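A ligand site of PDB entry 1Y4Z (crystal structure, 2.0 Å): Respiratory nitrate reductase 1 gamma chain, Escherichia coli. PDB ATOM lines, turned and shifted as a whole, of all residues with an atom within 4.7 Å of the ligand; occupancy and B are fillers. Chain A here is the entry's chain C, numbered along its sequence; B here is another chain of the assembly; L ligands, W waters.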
ATOM      1  N   ALA A  37      26.285   3.428 -18.236  1.00  0.00           N
ATOM      2  CA  ALA A  37      25.320   2.615 -18.954  1.00  0.00           C
ATOM      3  C   ALA A  37      25.163   1.226 -18.346  1.00  0.00           C
ATOM      4  O   ALA A  37      24.162   0.535 -18.556  1.00  0.00           O
ATOM      5  CB  ALA A  37      25.736   2.495 -20.418  1.00  0.00           C
ATOM      6  N   ALA A  38      26.167   0.834 -17.566  1.00  0.00           N
ATOM      7  CA  ALA A  38      26.166  -0.471 -16.936  1.00  0.00           C
ATOM      8  C   ALA A  38      26.041  -1.628 -17.908  1.00  0.00           C
ATOM      9  O   ALA A  38      25.183  -2.503 -17.757  1.00  0.00           O
ATOM     10  CB  ALA A  38      25.080  -0.548 -15.856  1.00  0.00           C
ATOM     11  N   SER A  39      26.906  -1.648 -18.899  1.00  0.00           N
ATOM     12  CA  SER A  39      26.925  -2.731 -19.859  1.00  0.00           C
ATOM     13  C   SER A  39      27.144  -4.060 -19.151  1.00  0.00           C
ATOM     14  O   SER A  39      27.901  -4.124 -18.189  1.00  0.00           O
ATOM     15  CB  SER A  39      28.066  -2.519 -20.844  1.00  0.00           C
ATOM     16  OG  SER A  39      28.184  -3.669 -21.680  1.00  0.00           O
ATOM     17  N   SER A  40      26.492  -5.120 -19.650  1.00  0.00           N
ATOM     18  CA  SER A  40      26.629  -6.440 -19.065  1.00  0.00           C
ATOM     19  C   SER A  40      27.046  -7.337 -20.206  1.00  0.00           C
ATOM     20  O   SER A  40      27.144  -8.551 -20.057  1.00  0.00           O
ATOM     21  CB  SER A  40      25.268  -6.914 -18.493  1.00  0.00           C
ATOM     22  OG  SER A  40      24.248  -6.986 -19.532  1.00  0.00           O
ATOM     23  N   GLN A  41      27.315  -6.713 -21.349  1.00  0.00           N
ATOM     24  CA  GLN A  41      27.658  -7.469 -22.548  1.00  0.00           C
ATOM     25  C   GLN A  41      28.823  -8.461 -22.399  1.00  0.00           C
ATOM     26  O   GLN A  41      28.744  -9.621 -22.861  1.00  0.00           O
ATOM     27  CB  GLN A  41      27.932  -6.492 -23.706  1.00  0.00           C
ATOM     28  CG  GLN A  41      27.766  -7.131 -25.085  1.00  0.00           C
ATOM     29  CD  GLN A  41      28.339  -6.281 -26.214  1.00  0.00           C
ATOM     30  OE1 GLN A  41      28.564  -5.077 -26.059  1.00  0.00           O
ATOM     31  NE2 GLN A  41      28.586  -6.902 -27.356  1.00  0.00           N
ATOM     32  N   MET A  48      22.956 -10.471 -27.489  1.00  0.00           N
ATOM     33  CA  MET A  48      22.960  -9.047 -27.199  1.00  0.00           C
ATOM     34  C   MET A  48      22.940  -8.151 -28.425  1.00  0.00           C
ATOM     35  O   MET A  48      22.336  -7.071 -28.419  1.00  0.00           O
ATOM     36  CB  MET A  48      24.175  -8.692 -26.322  1.00  0.00           C
ATOM     37  CG  MET A  48      23.898  -8.834 -24.846  1.00  0.00           C
ATOM     38  SD  MET A  48      22.496  -7.764 -24.380  1.00  0.00           S
ATOM     39  CE  MET A  48      23.252  -6.375 -23.691  1.00  0.00           C
ATOM     40  N   SER A  52      19.750  -5.894 -28.056  1.00  0.00           N
ATOM     41  CA  SER A  52      19.968  -4.481 -27.735  1.00  0.00           C
ATOM     42  C   SER A  52      19.692  -3.554 -28.932  1.00  0.00           C
ATOM     43  O   SER A  52      19.145  -2.432 -28.769  1.00  0.00           O
ATOM     44  CB  SER A  52      21.400  -4.245 -27.198  1.00  0.00           C
ATOM     45  OG  SER A  52      21.531  -2.911 -26.708  1.00  0.00           O
ATOM     46  N   PHE A  55      15.858  -3.426 -29.390  1.00  0.00           N
ATOM     47  CA  PHE A  55      15.344  -2.588 -28.353  1.00  0.00           C
ATOM     48  C   PHE A  55      15.685  -1.131 -28.536  1.00  0.00           C
ATOM     49  O   PHE A  55      14.781  -0.285 -28.485  1.00  0.00           O
ATOM     50  CB  PHE A  55      15.834  -3.076 -26.983  1.00  0.00           C
ATOM     51  CG  PHE A  55      15.459  -2.168 -25.870  1.00  0.00           C
ATOM     52  CD1 PHE A  55      16.345  -1.188 -25.411  1.00  0.00           C
ATOM     53  CD2 PHE A  55      14.185  -2.248 -25.301  1.00  0.00           C
ATOM     54  CE1 PHE A  55      15.968  -0.305 -24.396  1.00  0.00           C
ATOM     55  CE2 PHE A  55      13.797  -1.375 -24.297  1.00  0.00           C
ATOM     56  CZ  PHE A  55      14.683  -0.395 -23.837  1.00  0.00           C
ATOM     57  N   HIS A  56      16.959  -0.798 -28.759  1.00  0.00           N
ATOM     58  CA  HIS A  56      17.307   0.615 -28.852  1.00  0.00           C
ATOM     59  C   HIS A  56      16.800   1.298 -30.117  1.00  0.00           C
ATOM     60  O   HIS A  56      16.279   2.418 -30.056  1.00  0.00           O
ATOM     61  CB  HIS A  56      18.845   0.866 -28.663  1.00  0.00           C
ATOM     62  CG  HIS A  56      19.307   0.825 -27.206  1.00  0.00           C
ATOM     63  ND1 HIS A  56      19.786  -0.314 -26.598  1.00  0.00           N
ATOM     64  CD2 HIS A  56      19.282   1.781 -26.239  1.00  0.00           C
ATOM     65  CE1 HIS A  56      20.057  -0.054 -25.325  1.00  0.00           C
ATOM     66  NE2 HIS A  56      19.760   1.213 -25.069  1.00  0.00           N
ATOM     67  N   ILE A  59      12.981   1.764 -29.467  1.00  0.00           N
ATOM     68  CA  ILE A  59      12.652   2.812 -28.508  1.00  0.00           C
ATOM     69  C   ILE A  59      13.075   4.208 -28.944  1.00  0.00           C
ATOM     70  O   ILE A  59      12.509   5.226 -28.496  1.00  0.00           O
ATOM     71  CB  ILE A  59      13.262   2.505 -27.121  1.00  0.00           C
ATOM     72  CG1 ILE A  59      12.392   3.139 -26.039  1.00  0.00           C
ATOM     73  CG2 ILE A  59      14.678   3.094 -27.008  1.00  0.00           C
ATOM     74  CD1 ILE A  59      11.983   2.161 -24.936  1.00  0.00           C
ATOM     75  N   LEU A  60      14.086   4.304 -29.798  1.00  0.00           N
ATOM     76  CA  LEU A  60      14.499   5.627 -30.234  1.00  0.00           C
ATOM     77  C   LEU A  60      13.541   6.179 -31.302  1.00  0.00           C
ATOM     78  O   LEU A  60      13.324   7.391 -31.366  1.00  0.00           O
ATOM     79  CB  LEU A  60      15.966   5.629 -30.722  1.00  0.00           C
ATOM     80  CG  LEU A  60      16.964   5.605 -29.539  1.00  0.00           C
ATOM     81  CD1 LEU A  60      18.413   5.579 -30.032  1.00  0.00           C
ATOM     82  CD2 LEU A  60      16.753   6.839 -28.672  1.00  0.00           C
ATOM     83  N   LEU A 108      15.883  -9.017 -23.893  1.00  0.00           N
ATOM     84  CA  LEU A 108      16.797  -8.518 -22.860  1.00  0.00           C
ATOM     85  C   LEU A 108      16.326  -8.960 -21.492  1.00  0.00           C
ATOM     86  O   LEU A 108      17.132  -9.312 -20.653  1.00  0.00           O
ATOM     87  CB  LEU A 108      16.876  -6.990 -22.909  1.00  0.00           C
ATOM     88  CG  LEU A 108      17.531  -6.386 -24.158  1.00  0.00           C
ATOM     89  CD1 LEU A 108      17.264  -4.868 -24.243  1.00  0.00           C
ATOM     90  CD2 LEU A 108      19.038  -6.647 -24.140  1.00  0.00           C
ATOM     91  N   ARG A 111      16.981 -12.574 -20.839  1.00  0.00           N
ATOM     92  CA  ARG A 111      18.425 -12.674 -20.575  1.00  0.00           C
ATOM     93  C   ARG A 111      18.790 -12.246 -19.158  1.00  0.00           C
ATOM     94  O   ARG A 111      19.525 -12.962 -18.470  1.00  0.00           O
ATOM     95  CB  ARG A 111      19.210 -11.790 -21.540  1.00  0.00           C
ATOM     96  CG  ARG A 111      20.756 -11.795 -21.363  1.00  0.00           C
ATOM     97  CD  ARG A 111      21.383 -11.076 -22.548  1.00  0.00           C
ATOM     98  NE  ARG A 111      22.796 -10.740 -22.365  1.00  0.00           N
ATOM     99  CZ  ARG A 111      23.269  -9.798 -21.550  1.00  0.00           C
ATOM    100  NH1 ARG A 111      24.589  -9.603 -21.488  1.00  0.00           N
ATOM    101  NH2 ARG A 111      22.464  -9.028 -20.820  1.00  0.00           N
ATOM    102  N   ARG A 112      18.260 -11.100 -18.713  1.00  0.00           N
ATOM    103  CA  ARG A 112      18.590 -10.560 -17.412  1.00  0.00           C
ATOM    104  C   ARG A 112      18.130 -11.455 -16.312  1.00  0.00           C
ATOM    105  O   ARG A 112      18.790 -11.595 -15.268  1.00  0.00           O
ATOM    106  CB  ARG A 112      17.996  -9.137 -17.247  1.00  0.00           C
ATOM    107  CG  ARG A 112      18.333  -8.430 -15.881  1.00  0.00           C
ATOM    108  CD  ARG A 112      18.229  -6.902 -15.962  1.00  0.00           C
ATOM    109  NE  ARG A 112      19.208  -6.398 -16.920  1.00  0.00           N
ATOM    110  CZ  ARG A 112      20.542  -6.353 -16.701  1.00  0.00           C
ATOM    111  NH1 ARG A 112      21.044  -6.753 -15.527  1.00  0.00           N
ATOM    112  NH2 ARG A 112      21.371  -5.973 -17.667  1.00  0.00           N
ATOM    113  N   ILE A 129      13.256  -1.467 -13.878  1.00  0.00           N
ATOM    114  CA  ILE A 129      13.120  -0.487 -14.939  1.00  0.00           C
ATOM    115  C   ILE A 129      12.863  -1.136 -16.309  1.00  0.00           C
ATOM    116  O   ILE A 129      12.052  -0.639 -17.100  1.00  0.00           O
ATOM    117  CB  ILE A 129      14.354   0.491 -14.950  1.00  0.00           C
ATOM    118  CG1 ILE A 129      13.943   1.832 -15.525  1.00  0.00           C
ATOM    119  CG2 ILE A 129      15.492  -0.062 -15.787  1.00  0.00           C
ATOM    120  CD1 ILE A 129      13.192   2.724 -14.548  1.00  0.00           C
ATOM    121  N   LEU A 130      13.510  -2.264 -16.569  1.00  0.00           N
ATOM    122  CA  LEU A 130      13.362  -2.952 -17.823  1.00  0.00           C
ATOM    123  C   LEU A 130      11.983  -3.596 -17.890  1.00  0.00           C
ATOM    124  O   LEU A 130      11.324  -3.565 -18.931  1.00  0.00           O
ATOM    125  CB  LEU A 130      14.422  -4.045 -17.990  1.00  0.00           C
ATOM    126  CG  LEU A 130      14.279  -4.863 -19.276  1.00  0.00           C
ATOM    127  CD1 LEU A 130      14.339  -3.890 -20.481  1.00  0.00           C
ATOM    128  CD2 LEU A 130      15.393  -5.907 -19.396  1.00  0.00           C
ATOM    129  N   LEU A 133       9.488  -0.960 -18.788  1.00  0.00           N
ATOM    130  CA  LEU A 133       9.525  -0.472 -20.172  1.00  0.00           C
ATOM    131  C   LEU A 133       8.874  -1.529 -21.076  1.00  0.00           C
ATOM    132  O   LEU A 133       8.235  -1.188 -22.074  1.00  0.00           O
ATOM    133  CB  LEU A 133      10.965  -0.194 -20.636  1.00  0.00           C
ATOM    134  CG  LEU A 133      11.646   1.022 -20.044  1.00  0.00           C
ATOM    135  CD1 LEU A 133      13.135   0.810 -20.109  1.00  0.00           C
ATOM    136  CD2 LEU A 133      11.238   2.284 -20.795  1.00  0.00           C
ATOM    137  N   ARG A 202      19.434   3.142 -14.130  1.00  0.00           N
ATOM    138  CA  ARG A 202      20.436   3.257 -15.173  1.00  0.00           C
ATOM    139  C   ARG A 202      19.980   4.191 -16.328  1.00  0.00           C
ATOM    140  O   ARG A 202      20.800   4.541 -17.169  1.00  0.00           O
ATOM    141  CB  ARG A 202      20.701   1.886 -15.742  1.00  0.00           C
ATOM    142  CG  ARG A 202      19.490   1.327 -16.520  1.00  0.00           C
ATOM    143  CD  ARG A 202      19.609  -0.148 -16.762  1.00  0.00           C
ATOM    144  NE  ARG A 202      20.755  -0.429 -17.589  1.00  0.00           N
ATOM    145  CZ  ARG A 202      21.347  -1.622 -17.668  1.00  0.00           C
ATOM    146  NH1 ARG A 202      20.871  -2.651 -16.976  1.00  0.00           N
ATOM    147  NH2 ARG A 202      22.475  -1.749 -18.388  1.00  0.00           N
ATOM    148  N   LEU A 203      18.706   4.587 -16.359  1.00  0.00           N
ATOM    149  CA  LEU A 203      18.226   5.475 -17.430  1.00  0.00           C
ATOM    150  C   LEU A 203      18.995   6.772 -17.539  1.00  0.00           C
ATOM    151  O   LEU A 203      18.938   7.451 -18.564  1.00  0.00           O
ATOM    152  CB  LEU A 203      16.726   5.781 -17.269  1.00  0.00           C
ATOM    153  CG  LEU A 203      15.911   4.481 -17.315  1.00  0.00           C
ATOM    154  CD1 LEU A 203      14.470   4.832 -17.488  1.00  0.00           C
ATOM    155  CD2 LEU A 203      16.359   3.604 -18.468  1.00  0.00           C
ATOM    156  N   HIS A 205      21.830   7.156 -18.315  1.00  0.00           N
ATOM    157  CA  HIS A 205      22.729   7.058 -19.477  1.00  0.00           C
ATOM    158  C   HIS A 205      22.206   7.831 -20.668  1.00  0.00           C
ATOM    159  O   HIS A 205      22.987   8.330 -21.489  1.00  0.00           O
ATOM    160  CB  HIS A 205      23.029   5.605 -19.939  1.00  0.00           C
ATOM    161  CG  HIS A 205      21.900   4.874 -20.638  1.00  0.00           C
ATOM    162  ND1 HIS A 205      20.746   4.493 -19.984  1.00  0.00           N
ATOM    163  CD2 HIS A 205      21.842   4.302 -21.870  1.00  0.00           C
ATOM    164  CE1 HIS A 205      20.041   3.703 -20.770  1.00  0.00           C
ATOM    165  NE2 HIS A 205      20.677   3.556 -21.921  1.00  0.00           N
ATOM    166  N   ILE A 206      20.871   7.934 -20.732  1.00  0.00           N
ATOM    167  CA  ILE A 206      20.239   8.643 -21.858  1.00  0.00           C
ATOM    168  C   ILE A 206      20.730  10.102 -21.919  1.00  0.00           C
ATOM    169  O   ILE A 206      20.979  10.626 -23.011  1.00  0.00           O
ATOM    170  CB  ILE A 206      18.670   8.598 -21.756  1.00  0.00           C
ATOM    171  CG1 ILE A 206      18.179   7.153 -21.764  1.00  0.00           C
ATOM    172  CG2 ILE A 206      18.054   9.349 -22.945  1.00  0.00           C
ATOM    173  CD1 ILE A 206      16.777   6.967 -21.226  1.00  0.00           C
ATOM    174  N   VAL A 209      23.946  10.705 -24.283  1.00  0.00           N
ATOM    175  CA  VAL A 209      24.046  10.350 -25.727  1.00  0.00           C
ATOM    176  C   VAL A 209      25.257  11.197 -26.233  1.00  0.00           C
ATOM    177  O   VAL A 209      25.206  12.426 -26.220  1.00  0.00           O
ATOM    178  CB  VAL A 209      22.695  10.644 -26.463  1.00  0.00           C
ATOM    179  CG1 VAL A 209      22.243  12.052 -26.205  1.00  0.00           C
ATOM    180  CG2 VAL A 209      22.861  10.421 -27.980  1.00  0.00           C
ATOM    181  N   PRO A 210      26.359  10.542 -26.629  1.00  0.00           N
ATOM    182  CA  PRO A 210      27.631  11.136 -27.107  1.00  0.00           C
ATOM    183  C   PRO A 210      27.709  11.924 -28.409  1.00  0.00           C
ATOM    184  O   PRO A 210      28.588  11.694 -29.225  1.00  0.00           O
ATOM    185  CB  PRO A 210      28.594   9.937 -27.097  1.00  0.00           C
ATOM    186  CG  PRO A 210      27.736   8.813 -27.527  1.00  0.00           C
ATOM    187  CD  PRO A 210      26.325   9.099 -26.908  1.00  0.00           C
ATOM    188  N   ILE B  88      27.321   1.355 -30.889  1.00  0.00           N
ATOM    189  CA  ILE B  88      27.185   1.537 -29.448  1.00  0.00           C
ATOM    190  C   ILE B  88      26.159   0.730 -28.668  1.00  0.00           C
ATOM    191  O   ILE B  88      26.348   0.497 -27.474  1.00  0.00           O
ATOM    192  CB  ILE B  88      26.986   3.027 -29.129  1.00  0.00           C
ATOM    193  CG1 ILE B  88      27.523   3.327 -27.726  1.00  0.00           C
ATOM    194  CG2 ILE B  88      25.466   3.420 -29.287  1.00  0.00           C
ATOM    195  CD1 ILE B  88      27.911   4.753 -27.550  1.00  0.00           C
ATOM    196  N   PHE B  89      25.077   0.256 -29.281  1.00  0.00           N
ATOM    197  CA  PHE B  89      24.100  -0.460 -28.467  1.00  0.00           C
ATOM    198  C   PHE B  89      24.586  -1.835 -28.091  1.00  0.00           C
ATOM    199  O   PHE B  89      24.119  -2.400 -27.109  1.00  0.00           O
ATOM    200  CB  PHE B  89      22.748  -0.543 -29.189  1.00  0.00           C
ATOM    201  CG  PHE B  89      22.208   0.797 -29.562  1.00  0.00           C
ATOM    202  CD1 PHE B  89      22.142   1.802 -28.629  1.00  0.00           C
ATOM    203  CD2 PHE B  89      21.799   1.056 -30.867  1.00  0.00           C
ATOM    204  CE1 PHE B  89      21.688   3.070 -28.954  1.00  0.00           C
ATOM    205  CE2 PHE B  89      21.334   2.330 -31.228  1.00  0.00           C
ATOM    206  CZ  PHE B  89      21.286   3.345 -30.273  1.00  0.00           C
ATOM    207  N   TRP B 220      30.557   3.293 -22.213  1.00  0.00           N
ATOM    208  CA  TRP B 220      30.194   2.950 -23.593  1.00  0.00           C
ATOM    209  C   TRP B 220      30.978   1.749 -24.083  1.00  0.00           C
ATOM    210  O   TRP B 220      30.617   1.113 -25.082  1.00  0.00           O
ATOM    211  CB  TRP B 220      30.469   4.119 -24.515  1.00  0.00           C
ATOM    212  CG  TRP B 220      29.688   5.392 -24.165  1.00  0.00           C
ATOM    213  CD1 TRP B 220      30.187   6.656 -24.130  1.00  0.00           C
ATOM    214  CD2 TRP B 220      28.277   5.516 -23.834  1.00  0.00           C
ATOM    215  NE1 TRP B 220      29.210   7.546 -23.798  1.00  0.00           N
ATOM    216  CE2 TRP B 220      28.025   6.879 -23.611  1.00  0.00           C
ATOM    217  CE3 TRP B 220      27.224   4.601 -23.715  1.00  0.00           C
ATOM    218  CZ2 TRP B 220      26.748   7.383 -23.273  1.00  0.00           C
ATOM    219  CZ3 TRP B 220      25.931   5.089 -23.374  1.00  0.00           C
ATOM    220  CH2 TRP B 220      25.721   6.466 -23.170  1.00  0.00           C
ATOM    221  N   ARG B 221      32.039   1.399 -23.359  1.00  0.00           N
ATOM    222  CA  ARG B 221      32.874   0.235 -23.681  1.00  0.00           C
ATOM    223  C   ARG B 221      33.290  -0.006 -25.149  1.00  0.00           C
ATOM    224  O   ARG B 221      33.305  -1.147 -25.623  1.00  0.00           O
ATOM    225  CB  ARG B 221      32.259  -1.043 -23.083  1.00  0.00           C
ATOM    226  CG  ARG B 221      30.750  -1.333 -23.382  1.00  0.00           C
ATOM    227  CD  ARG B 221      30.574  -2.044 -24.718  1.00  0.00           C
ATOM    228  NE  ARG B 221      29.176  -2.407 -24.986  1.00  0.00           N
ATOM    229  CZ  ARG B 221      28.285  -1.595 -25.551  1.00  0.00           C
ATOM    230  NH1 ARG B 221      28.640  -0.358 -25.895  1.00  0.00           N
ATOM    231  NH2 ARG B 221      27.029  -2.017 -25.774  1.00  0.00           N
HETATM  232  C1  LIG L   1      21.415  -0.343 -21.961  1.00  0.00           C
HETATM  233  C2  LIG L   1      23.326   2.984 -24.861  1.00  0.00           C
HETATM  234  C3  LIG L   1      18.989   5.162 -25.051  1.00  0.00           C
HETATM  235  C4  LIG L   1      17.158   1.878 -22.087  1.00  0.00           C
HETATM  236  C5  LIG L   1      22.312   0.358 -22.730  1.00  0.00           C
HETATM  237  C6  LIG L   1      23.714   0.041 -22.937  1.00  0.00           C
HETATM  238  C7  LIG L   1      24.252   0.967 -23.734  1.00  0.00           C
HETATM  239  C8  LIG L   1      23.186   1.881 -24.054  1.00  0.00           C
HETATM  240  C9  LIG L   1      25.713   1.131 -24.276  1.00  0.00           C
HETATM  241  C10 LIG L   1      24.388  -1.148 -22.310  1.00  0.00           C
HETATM  242  C11 LIG L   1      24.149  -2.454 -23.170  1.00  0.00           C
HETATM  243  C12 LIG L   1      25.107  -3.602 -22.762  1.00  0.00           C
HETATM  244  O1  LIG L   1      26.190  -3.707 -23.412  1.00  0.00           O
HETATM  245  O2  LIG L   1      24.762  -4.306 -21.778  1.00  0.00           O
HETATM  246  C13 LIG L   1      22.305   3.873 -25.175  1.00  0.00           C
HETATM  247  C14 LIG L   1      22.459   5.058 -26.027  1.00  0.00           C
HETATM  248  C15 LIG L   1      21.233   5.664 -26.063  1.00  0.00           C
HETATM  249  C16 LIG L   1      20.321   4.869 -25.256  1.00  0.00           C
HETATM  250  C17 LIG L   1      23.815   5.482 -26.713  1.00  0.00           C
HETATM  251  C18 LIG L   1      20.827   6.968 -26.818  1.00  0.00           C
HETATM  252  C19 LIG L   1      21.288   7.320 -28.041  1.00  0.00           C
HETATM  253  C20 LIG L   1      18.090   4.464 -24.272  1.00  0.00           C
HETATM  254  C21 LIG L   1      16.684   4.804 -24.063  1.00  0.00           C
HETATM  255  C22 LIG L   1      16.185   3.878 -23.216  1.00  0.00           C
HETATM  256  C23 LIG L   1      17.277   2.962 -22.913  1.00  0.00           C
HETATM  257  C24 LIG L   1      15.983   6.044 -24.742  1.00  0.00           C
HETATM  258  C25 LIG L   1      14.770   3.656 -22.584  1.00  0.00           C
HETATM  259  C26 LIG L   1      14.121   4.725 -22.050  1.00  0.00           C
HETATM  260  C27 LIG L   1      18.140   0.987 -21.789  1.00  0.00           C
HETATM  261  C28 LIG L   1      17.972  -0.156 -20.921  1.00  0.00           C
HETATM  262  C29 LIG L   1      19.165  -0.791 -20.913  1.00  0.00           C
HETATM  263  C30 LIG L   1      20.090  -0.020 -21.753  1.00  0.00           C
HETATM  264  C31 LIG L   1      16.655  -0.547 -20.186  1.00  0.00           C
HETATM  265  C32 LIG L   1      19.602  -2.121 -20.177  1.00  0.00           C
HETATM  266  C33 LIG L   1      19.079  -3.439 -20.869  1.00  0.00           C
HETATM  267  C34 LIG L   1      19.323  -4.708 -20.027  1.00  0.00           C
HETATM  268  O3  LIG L   1      20.252  -5.476 -20.417  1.00  0.00           O
HETATM  269  O4  LIG L   1      18.543  -4.864 -19.017  1.00  0.00           O
HETATM  270  N1  LIG L   1      22.013   1.489 -23.421  1.00  0.00           N
HETATM  271  N2  LIG L   1      20.992   3.778 -24.715  1.00  0.00           N
HETATM  272  N3  LIG L   1      18.415   3.328 -23.564  1.00  0.00           N
HETATM  273  N4  LIG L   1      19.460   1.040 -22.277  1.00  0.00           N
HETATM  274 FE1  LIG L   1      20.237   2.381 -23.507  1.00  0.00          FE
HETATM  275  O   HOH W   1      21.682   1.482 -19.528  1.00  0.00           O
HETATM  276  O   HOH W   2      19.855  -8.230 -20.521  1.00  0.00           O
HETATM  277  O   HOH W   3      22.860  -4.558 -20.019  1.00  0.00           O
HETATM  278  O   HOH W   4      17.916  -3.095 -17.266  1.00  0.00           O
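NE2 of His 56 binds FE1 of the ligand, 2.0 Å away. NE2 of His 205 binds FE1 of the ligand, at 2.0 Å. The side-chain hydroxyl (OG) of Ser 39 is in hydrogen-bond range of an oxygen (O1) of the ligand (2.6 Å). O4 of the ligand is in salt-bridge range of NE of Arg 112 (2.7 Å). O2 of the ligand is in hydrogen-bond range of N of Ser 40 (2.9 Å). An oxygen (O1) of the ligand lies within salt-bridge range of the guanidinium group (NH2) of Arg 221 of chain B, at 3.0 Å. The guanidinium group (NH1) of Arg 202 is in salt-bridge range of an oxygen (O4) of the ligand, at 3.8 Å.
ND1 of His 56 lies within hydrogen-bond range of O of Ser 52. O of Arg 202 sits at hydrogen-bond distance from ND1 of His 205, 2.8 Å away. The guanidinium group of Arg 221 of chain B is in hydrogen-bond range of the backbone carbonyl oxygen of Ile 88 of chain B. The guanidinium group (NH2) of Arg 221 of chain B sits at hydrogen-bond distance from the backbone carbonyl oxygen (O) of Phe 89 of chain B (3.2 Å). NH2 of Arg 202 sits at hydrogen-bond distance from O of Ala 37, 2.8 Å away. The guanidinium group (NH2) of Arg 202 is in hydrogen-bond range of the backbone carbonyl oxygen (O) of Ala 38 (2.9 Å). The side-chain sulfur (SD) of Met 48 lies close to the guanidinium group (NE) of Arg 111, 3.6 Å away. The side-chain hydroxyl (OG) of Ser 52 is in hydrogen-bond range of the backbone carbonyl oxygen (O) of Phe 89 of chain B (2.7 Å).
Residues that only touch the ligand: Met 48 (3.2 Å), Gln 41 (3.3 Å), Ile 88 of chain B (3.3 Å), Leu 130 (3.3 Å), Phe 55 (3.4 Å), Val 209 (3.5 Å), Ile 206 (3.6 Å), Phe 89 of chain B (3.6 Å), Trp 220 of chain B (3.7 Å), Leu 133 (3.8 Å), Leu 60 (3.9 Å), Ala 37 (3.9 Å) and Ile 59 (3.9 Å). Hydrophobic or aromatic side chains that line the ligand: Ala 37, Met 48, Phe 55, His 56, Ile 59, Leu 60, Leu 130, Leu 133, His 205, Ile 206, Val 209, Ile 88 of chain B, Phe 89 of chain B and Trp 220 of chain B. Of the 27 residues printed, 20 come within 4 Å of the ligand. The nearest printed residue that does not touch the ligand is Leu 108 (4.1 Å).
Water W4 bridges O4 of the ligand (2.6 Å) and NH1 of Arg 202 (3.0 Å). Water W3 lies within hydrogen-bond range of an oxygen (O2) of the ligand (2.6 Å), the side-chain hydroxyl (OG) of Ser 40 (2.8 Å), the guanidinium group (NH2) of Arg 112 (3.1 Å) and the guanidinium group (NH2) of Arg 202 (3.3 Å). Water W2 lies within hydrogen-bond range of NH2 of Arg 111, O3 of the ligand and O of Leu 108. Water W1 lies within hydrogen-bond range of the backbone carbonyl oxygen of Ala 37 (2.8 Å), the guanidinium group of Arg 202 (2.9 Å) and a ring nitrogen (ND1) of His 205 (3.2 Å).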
